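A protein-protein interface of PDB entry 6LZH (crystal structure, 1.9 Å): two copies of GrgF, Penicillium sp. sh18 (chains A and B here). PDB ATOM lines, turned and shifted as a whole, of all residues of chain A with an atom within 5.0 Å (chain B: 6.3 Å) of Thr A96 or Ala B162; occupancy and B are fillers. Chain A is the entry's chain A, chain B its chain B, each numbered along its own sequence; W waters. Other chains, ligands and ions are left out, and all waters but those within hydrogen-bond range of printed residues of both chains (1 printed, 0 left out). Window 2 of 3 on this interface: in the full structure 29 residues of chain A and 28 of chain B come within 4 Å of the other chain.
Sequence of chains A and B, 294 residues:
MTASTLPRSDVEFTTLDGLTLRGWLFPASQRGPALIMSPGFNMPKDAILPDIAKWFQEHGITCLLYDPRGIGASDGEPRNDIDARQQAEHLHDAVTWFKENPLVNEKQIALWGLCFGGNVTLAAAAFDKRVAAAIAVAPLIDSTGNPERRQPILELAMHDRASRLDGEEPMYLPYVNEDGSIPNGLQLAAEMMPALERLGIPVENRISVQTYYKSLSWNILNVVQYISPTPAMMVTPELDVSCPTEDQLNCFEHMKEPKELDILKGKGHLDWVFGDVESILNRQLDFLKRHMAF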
ATOM      1  N   HIS A  92      -0.318   2.606  10.870  1.00  0.00           N
ATOM      2  CA  HIS A  92      -0.671   1.464  10.021  1.00  0.00           C
ATOM      3  C   HIS A  92       0.572   0.877   9.347  1.00  0.00           C
ATOM      4  O   HIS A  92       0.701  -0.344   9.200  1.00  0.00           O
ATOM      5  CB  HIS A  92      -1.679   1.866   8.942  1.00  0.00           C
ATOM      6  CG  HIS A  92      -2.855   2.649   9.440  1.00  0.00           C
ATOM      7  ND1 HIS A  92      -3.394   2.474  10.698  1.00  0.00           N
ATOM      8  CD2 HIS A  92      -3.594   3.618   8.843  1.00  0.00           C
ATOM      9  CE1 HIS A  92      -4.423   3.294  10.851  1.00  0.00           C
ATOM     10  NE2 HIS A  92      -4.570   3.994   9.737  1.00  0.00           N
ATOM     11  N   ASP A  93       1.493   1.734   8.915  1.00  0.00           N
ATOM     12  CA  ASP A  93       2.721   1.233   8.306  1.00  0.00           C
ATOM     13  C   ASP A  93       3.595   0.549   9.351  1.00  0.00           C
ATOM     14  O   ASP A  93       4.266  -0.453   9.057  1.00  0.00           O
ATOM     15  CB  ASP A  93       3.480   2.382   7.623  1.00  0.00           C
ATOM     16  CG  ASP A  93       2.700   2.978   6.461  1.00  0.00           C
ATOM     17  OD1 ASP A  93       1.811   2.267   5.940  1.00  0.00           O
ATOM     18  OD2 ASP A  93       2.967   4.159   6.083  1.00  0.00           O
ATOM     19  N   ALA A  94       3.573   1.055  10.581  1.00  0.00           N
ATOM     20  CA  ALA A  94       4.311   0.400  11.657  1.00  0.00           C
ATOM     21  C   ALA A  94       3.742  -0.986  11.951  1.00  0.00           C
ATOM     22  O   ALA A  94       4.500  -1.946  12.132  1.00  0.00           O
ATOM     23  CB  ALA A  94       4.284   1.282  12.909  1.00  0.00           C
ATOM     24  N   VAL A  95       2.408  -1.114  11.983  1.00  0.00           N
ATOM     25  CA  VAL A  95       1.787  -2.423  12.201  1.00  0.00           C
ATOM     26  C   VAL A  95       2.201  -3.392  11.090  1.00  0.00           C
ATOM     27  O   VAL A  95       2.571  -4.542  11.354  1.00  0.00           O
ATOM     28  CB  VAL A  95       0.254  -2.275  12.291  1.00  0.00           C
ATOM     29  CG1 VAL A  95      -0.453  -3.629  12.069  1.00  0.00           C
ATOM     30  CG2 VAL A  95      -0.171  -1.637  13.616  1.00  0.00           C
ATOM     31  N   THR A  96       2.154  -2.932   9.835  1.00  0.00           N
ATOM     32  CA  THR A  96       2.592  -3.741   8.693  1.00  0.00           C
ATOM     33  C   THR A  96       4.013  -4.248   8.886  1.00  0.00           C
ATOM     34  O   THR A  96       4.289  -5.440   8.712  1.00  0.00           O
ATOM     35  CB  THR A  96       2.502  -2.912   7.410  1.00  0.00           C
ATOM     36  OG1 THR A  96       1.137  -2.565   7.176  1.00  0.00           O
ATOM     37  CG2 THR A  96       3.065  -3.677   6.206  1.00  0.00           C
ATOM     38  N   TRP A  97       4.928  -3.340   9.224  1.00  0.00           N
ATOM     39  CA  TRP A  97       6.312  -3.714   9.513  1.00  0.00           C
ATOM     40  C   TRP A  97       6.394  -4.725  10.652  1.00  0.00           C
ATOM     41  O   TRP A  97       7.076  -5.756  10.546  1.00  0.00           O
ATOM     42  CB  TRP A  97       7.101  -2.448   9.863  1.00  0.00           C
ATOM     43  CG  TRP A  97       8.518  -2.673  10.221  1.00  0.00           C
ATOM     44  CD1 TRP A  97       9.563  -2.860   9.362  1.00  0.00           C
ATOM     45  CD2 TRP A  97       9.071  -2.714  11.545  1.00  0.00           C
ATOM     46  NE1 TRP A  97      10.737  -3.027  10.075  1.00  0.00           N
ATOM     47  CE2 TRP A  97      10.456  -2.939  11.414  1.00  0.00           C
ATOM     48  CE3 TRP A  97       8.526  -2.581  12.825  1.00  0.00           C
ATOM     49  CZ2 TRP A  97      11.303  -3.040  12.517  1.00  0.00           C
ATOM     50  CZ3 TRP A  97       9.367  -2.677  13.923  1.00  0.00           C
ATOM     51  CH2 TRP A  97      10.741  -2.903  13.760  1.00  0.00           C
ATOM     52  N   PHE A  98       5.709  -4.437  11.765  1.00  0.00           N
ATOM     53  CA  PHE A  98       5.894  -5.227  12.977  1.00  0.00           C
ATOM     54  C   PHE A  98       5.449  -6.665  12.785  1.00  0.00           C
ATOM     55  O   PHE A  98       6.069  -7.586  13.337  1.00  0.00           O
ATOM     56  CB  PHE A  98       5.122  -4.594  14.147  1.00  0.00           C
ATOM     57  CG  PHE A  98       5.769  -4.831  15.471  1.00  0.00           C
ATOM     58  CD1 PHE A  98       6.894  -5.633  15.519  1.00  0.00           C
ATOM     59  CD2 PHE A  98       5.309  -4.250  16.636  1.00  0.00           C
ATOM     60  CE1 PHE A  98       7.544  -5.873  16.689  1.00  0.00           C
ATOM     61  CE2 PHE A  98       5.979  -4.494  17.849  1.00  0.00           C
ATOM     62  CZ  PHE A  98       7.092  -5.314  17.850  1.00  0.00           C
ATOM     63  N   LYS A  99       4.397  -6.867  11.986  1.00  0.00           N
ATOM     64  CA  LYS A  99       3.869  -8.200  11.748  1.00  0.00           C
ATOM     65  C   LYS A  99       4.924  -9.157  11.193  1.00  0.00           C
ATOM     66  O   LYS A  99       4.807 -10.378  11.368  1.00  0.00           O
ATOM     67  CB  LYS A  99       2.684  -8.112  10.791  1.00  0.00           C
ATOM     68  CG  LYS A  99       1.358  -7.863  11.483  1.00  0.00           C
ATOM     69  CD  LYS A  99       0.305  -7.381  10.516  1.00  0.00           C
ATOM     70  CE  LYS A  99       0.218  -8.254   9.281  1.00  0.00           C
ATOM     71  NZ  LYS A  99      -1.130  -8.142   8.651  1.00  0.00           N
ATOM     72  N   GLU A 100       5.955  -8.635  10.524  1.00  0.00           N
ATOM     73  CA  GLU A 100       6.984  -9.502   9.965  1.00  0.00           C
ATOM     74  C   GLU A 100       8.005  -9.957  10.997  1.00  0.00           C
ATOM     75  O   GLU A 100       8.843 -10.810  10.683  1.00  0.00           O
ATOM     76  CB  GLU A 100       7.688  -8.800   8.802  1.00  0.00           C
ATOM     77  CG  GLU A 100       6.778  -8.554   7.610  1.00  0.00           C
ATOM     78  CD  GLU A 100       6.321  -9.853   6.931  1.00  0.00           C
ATOM     79  OE1 GLU A 100       7.179 -10.562   6.347  1.00  0.00           O
ATOM     80  OE2 GLU A 100       5.106 -10.154   6.968  1.00  0.00           O
ATOM     81  N   ARG A 130      -6.447  -4.660  12.151  1.00  0.00           N
ATOM     82  CA  ARG A 130      -5.339  -5.534  12.511  1.00  0.00           C
ATOM     83  C   ARG A 130      -4.837  -5.265  13.923  1.00  0.00           C
ATOM     84  O   ARG A 130      -4.098  -6.086  14.468  1.00  0.00           O
ATOM     85  CB  ARG A 130      -4.182  -5.379  11.518  1.00  0.00           C
ATOM     86  CG  ARG A 130      -4.596  -5.626  10.047  1.00  0.00           C
ATOM     87  CD  ARG A 130      -3.483  -5.200   9.099  1.00  0.00           C
ATOM     88  NE  ARG A 130      -3.137  -3.794   9.305  1.00  0.00           N
ATOM     89  CZ  ARG A 130      -2.033  -3.219   8.838  1.00  0.00           C
ATOM     90  NH1 ARG A 130      -1.162  -3.926   8.112  1.00  0.00           N
ATOM     91  NH2 ARG A 130      -1.808  -1.932   9.093  1.00  0.00           N
ATOM     92  N   ALA B 157      -8.450  -0.807   2.502  1.00  0.00           N
ATOM     93  CA  ALA B 157      -7.499   0.290   2.618  1.00  0.00           C
ATOM     94  C   ALA B 157      -6.235  -0.166   3.333  1.00  0.00           C
ATOM     95  O   ALA B 157      -5.117   0.092   2.867  1.00  0.00           O
ATOM     96  CB  ALA B 157      -8.143   1.460   3.354  1.00  0.00           C
ATOM     97  N   MET B 158      -6.396  -0.863   4.464  1.00  0.00           N
ATOM     98  CA  MET B 158      -5.238  -1.433   5.145  1.00  0.00           C
ATOM     99  C   MET B 158      -4.470  -2.371   4.221  1.00  0.00           C
ATOM    100  O   MET B 158      -3.237  -2.384   4.225  1.00  0.00           O
ATOM    101  CB  MET B 158      -5.672  -2.152   6.431  1.00  0.00           C
ATOM    102  CG  MET B 158      -6.140  -1.226   7.552  1.00  0.00           C
ATOM    103  SD  MET B 158      -4.990   0.132   7.897  1.00  0.00           S
ATOM    104  CE  MET B 158      -5.802   1.531   7.135  1.00  0.00           C
ATOM    105  N   HIS B 159      -5.170  -3.147   3.398  1.00  0.00           N
ATOM    106  CA  HIS B 159      -4.443  -4.092   2.561  1.00  0.00           C
ATOM    107  C   HIS B 159      -3.734  -3.395   1.402  1.00  0.00           C
ATOM    108  O   HIS B 159      -2.644  -3.805   0.988  1.00  0.00           O
ATOM    109  CB  HIS B 159      -5.339  -5.165   1.979  1.00  0.00           C
ATOM    110  CG  HIS B 159      -4.548  -6.383   1.615  1.00  0.00           C
ATOM    111  ND1 HIS B 159      -4.524  -6.898   0.338  1.00  0.00           N
ATOM    112  CD2 HIS B 159      -3.685  -7.136   2.345  1.00  0.00           C
ATOM    113  CE1 HIS B 159      -3.727  -7.950   0.304  1.00  0.00           C
ATOM    114  NE2 HIS B 159      -3.187  -8.100   1.501  1.00  0.00           N
ATOM    115  N   ASP B 160      -4.369  -2.367   0.833  1.00  0.00           N
ATOM    116  CA  ASP B 160      -3.742  -1.544  -0.189  1.00  0.00           C
ATOM    117  C   ASP B 160      -2.418  -0.959   0.307  1.00  0.00           C
ATOM    118  O   ASP B 160      -1.416  -0.956  -0.422  1.00  0.00           O
ATOM    119  CB  ASP B 160      -4.739  -0.471  -0.605  1.00  0.00           C
ATOM    120  CG  ASP B 160      -4.172   0.449  -1.665  1.00  0.00           C
ATOM    121  OD1 ASP B 160      -3.718  -0.065  -2.700  1.00  0.00           O
ATOM    122  OD2 ASP B 160      -4.223   1.676  -1.427  1.00  0.00           O
ATOM    123  N   ARG B 161      -2.400  -0.421   1.538  1.00  0.00           N
ATOM    124  CA  ARG B 161      -1.168   0.144   2.075  1.00  0.00           C
ATOM    125  C   ARG B 161      -0.053  -0.888   2.080  1.00  0.00           C
ATOM    126  O   ARG B 161       1.060  -0.623   1.613  1.00  0.00           O
ATOM    127  CB  ARG B 161      -1.373   0.652   3.505  1.00  0.00           C
ATOM    128  CG  ARG B 161      -2.154   1.909   3.683  1.00  0.00           C
ATOM    129  CD  ARG B 161      -2.010   2.394   5.145  1.00  0.00           C
ATOM    130  NE  ARG B 161      -0.765   3.134   5.337  1.00  0.00           N
ATOM    131  CZ  ARG B 161      -0.658   4.435   5.102  1.00  0.00           C
ATOM    132  NH1 ARG B 161      -1.725   5.114   4.667  1.00  0.00           N
ATOM    133  NH2 ARG B 161       0.499   5.058   5.277  1.00  0.00           N
ATOM    134  N   ALA B 162      -0.336  -2.070   2.630  1.00  0.00           N
ATOM    135  CA  ALA B 162       0.694  -3.099   2.742  1.00  0.00           C
ATOM    136  C   ALA B 162       1.147  -3.574   1.368  1.00  0.00           C
ATOM    137  O   ALA B 162       2.343  -3.800   1.149  1.00  0.00           O
ATOM    138  CB  ALA B 162       0.172  -4.269   3.571  1.00  0.00           C
ATOM    139  N   SER B 163       0.203  -3.707   0.423  1.00  0.00           N
ATOM    140  CA  SER B 163       0.543  -4.156  -0.928  1.00  0.00           C
ATOM    141  C   SER B 163       1.397  -3.129  -1.658  1.00  0.00           C
ATOM    142  O   SER B 163       2.380  -3.479  -2.321  1.00  0.00           O
ATOM    143  CB  SER B 163      -0.736  -4.437  -1.720  1.00  0.00           C
ATOM    144  OG  SER B 163      -1.456  -5.502  -1.136  1.00  0.00           O
ATOM    145  N   ARG B 164       1.032  -1.850  -1.561  1.00  0.00           N
ATOM    146  CA  ARG B 164       1.804  -0.818  -2.248  1.00  0.00           C
ATOM    147  C   ARG B 164       3.219  -0.725  -1.700  1.00  0.00           C
ATOM    148  O   ARG B 164       4.172  -0.474  -2.449  1.00  0.00           O
ATOM    149  CB  ARG B 164       1.101   0.531  -2.136  1.00  0.00           C
ATOM    150  CG  ARG B 164      -0.082   0.652  -3.065  1.00  0.00           C
ATOM    151  CD  ARG B 164      -1.031   1.721  -2.568  1.00  0.00           C
ATOM    152  NE  ARG B 164      -0.443   3.055  -2.651  1.00  0.00           N
ATOM    153  CZ  ARG B 164      -1.059   4.151  -2.222  1.00  0.00           C
ATOM    154  NH1 ARG B 164      -2.275   4.059  -1.695  1.00  0.00           N
ATOM    155  NH2 ARG B 164      -0.461   5.332  -2.306  1.00  0.00           N
ATOM    156  N   LEU B 165       3.376  -0.927  -0.391  1.00  0.00           N
ATOM    157  CA  LEU B 165       4.709  -0.988   0.189  1.00  0.00           C
ATOM    158  C   LEU B 165       5.522  -2.128  -0.412  1.00  0.00           C
ATOM    159  O   LEU B 165       6.753  -2.029  -0.508  1.00  0.00           O
ATOM    160  CB  LEU B 165       4.607  -1.143   1.705  1.00  0.00           C
ATOM    161  CG  LEU B 165       4.306   0.152   2.474  1.00  0.00           C
ATOM    162  CD1 LEU B 165       3.889  -0.169   3.899  1.00  0.00           C
ATOM    163  CD2 LEU B 165       5.501   1.083   2.455  1.00  0.00           C
ATOM    164  N   ASP B 166       4.856  -3.214  -0.819  1.00  0.00           N
ATOM    165  CA  ASP B 166       5.526  -4.366  -1.416  1.00  0.00           C
ATOM    166  C   ASP B 166       5.821  -4.169  -2.898  1.00  0.00           C
ATOM    167  O   ASP B 166       6.275  -5.108  -3.556  1.00  0.00           O
ATOM    168  CB  ASP B 166       4.684  -5.641  -1.218  1.00  0.00           C
ATOM    169  CG  ASP B 166       4.698  -6.150   0.224  1.00  0.00           C
ATOM    170  OD1 ASP B 166       5.614  -5.791   0.973  1.00  0.00           O
ATOM    171  OD2 ASP B 166       3.781  -6.904   0.624  1.00  0.00           O
ATOM    172  N   GLY B 167       5.581  -2.984  -3.445  1.00  0.00           N
ATOM    173  CA  GLY B 167       5.788  -2.739  -4.854  1.00  0.00           C
ATOM    174  C   GLY B 167       4.542  -2.874  -5.702  1.00  0.00           C
ATOM    175  O   GLY B 167       4.581  -2.543  -6.894  1.00  0.00           O
HETATM  176  O   HOH W   1      -2.191  -1.109   6.255  1.00  0.00           O
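OD2 of Asp A93 lies within salt-bridge range of NH2 of Arg B161, at 2.7 Å.
The backbone carbonyl oxygen (O) of His A92 sits at hydrogen-bond distance from the side-chain hydroxyl (OG1) of Thr A96 (3.0 Å). O of His A92 is in hydrogen-bond range of NH2 of Arg A130 (3.0 Å). The side-chain hydroxyl (OG1) of Thr A96 lies within hydrogen-bond range of the guanidinium group (NH1) of Arg A130 (2.8 Å).
Among the printed residues, pairs that only touch across the chains: His A92 with Met B158, Asp A93 with Leu B165, His A92 with Arg B161, Thr A96 with Ala B162 and Arg A130 with Met B158.
Printed residues of chain B within 4 Å of Thr A96: Ala B162. Of the printed residues of chain A, Arg B161 touches His A92 (3.8 Å) and Asp A93 (2.7 Å). Of the printed residues of chain B, Asp A93 touches Arg B161 and Leu B165. Arg B164 touches none of the printed residues of chain A. The nearest residue of chain A that does not touch Ala B162 is Arg A130 (4.7 Å).
Hydrophobic or aromatic side chains of chain B that line the printed part of chain A: Met B158, Ala B162 and Leu B165. Of the 10 printed residues of chain A, 4 touch a printed residue of chain B. Among the printed residues, 6 pairs touch across the chains.
No position is printed for both chains. Of the 6 pairs that touch across the chains among the printed residues, none has its exchanged pair printed and touching as well.
Water W1 bridges the backbone carbonyl oxygen of Met B158 (2.6 Å) and the guanidinium group of Arg A130 (3.0 Å).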
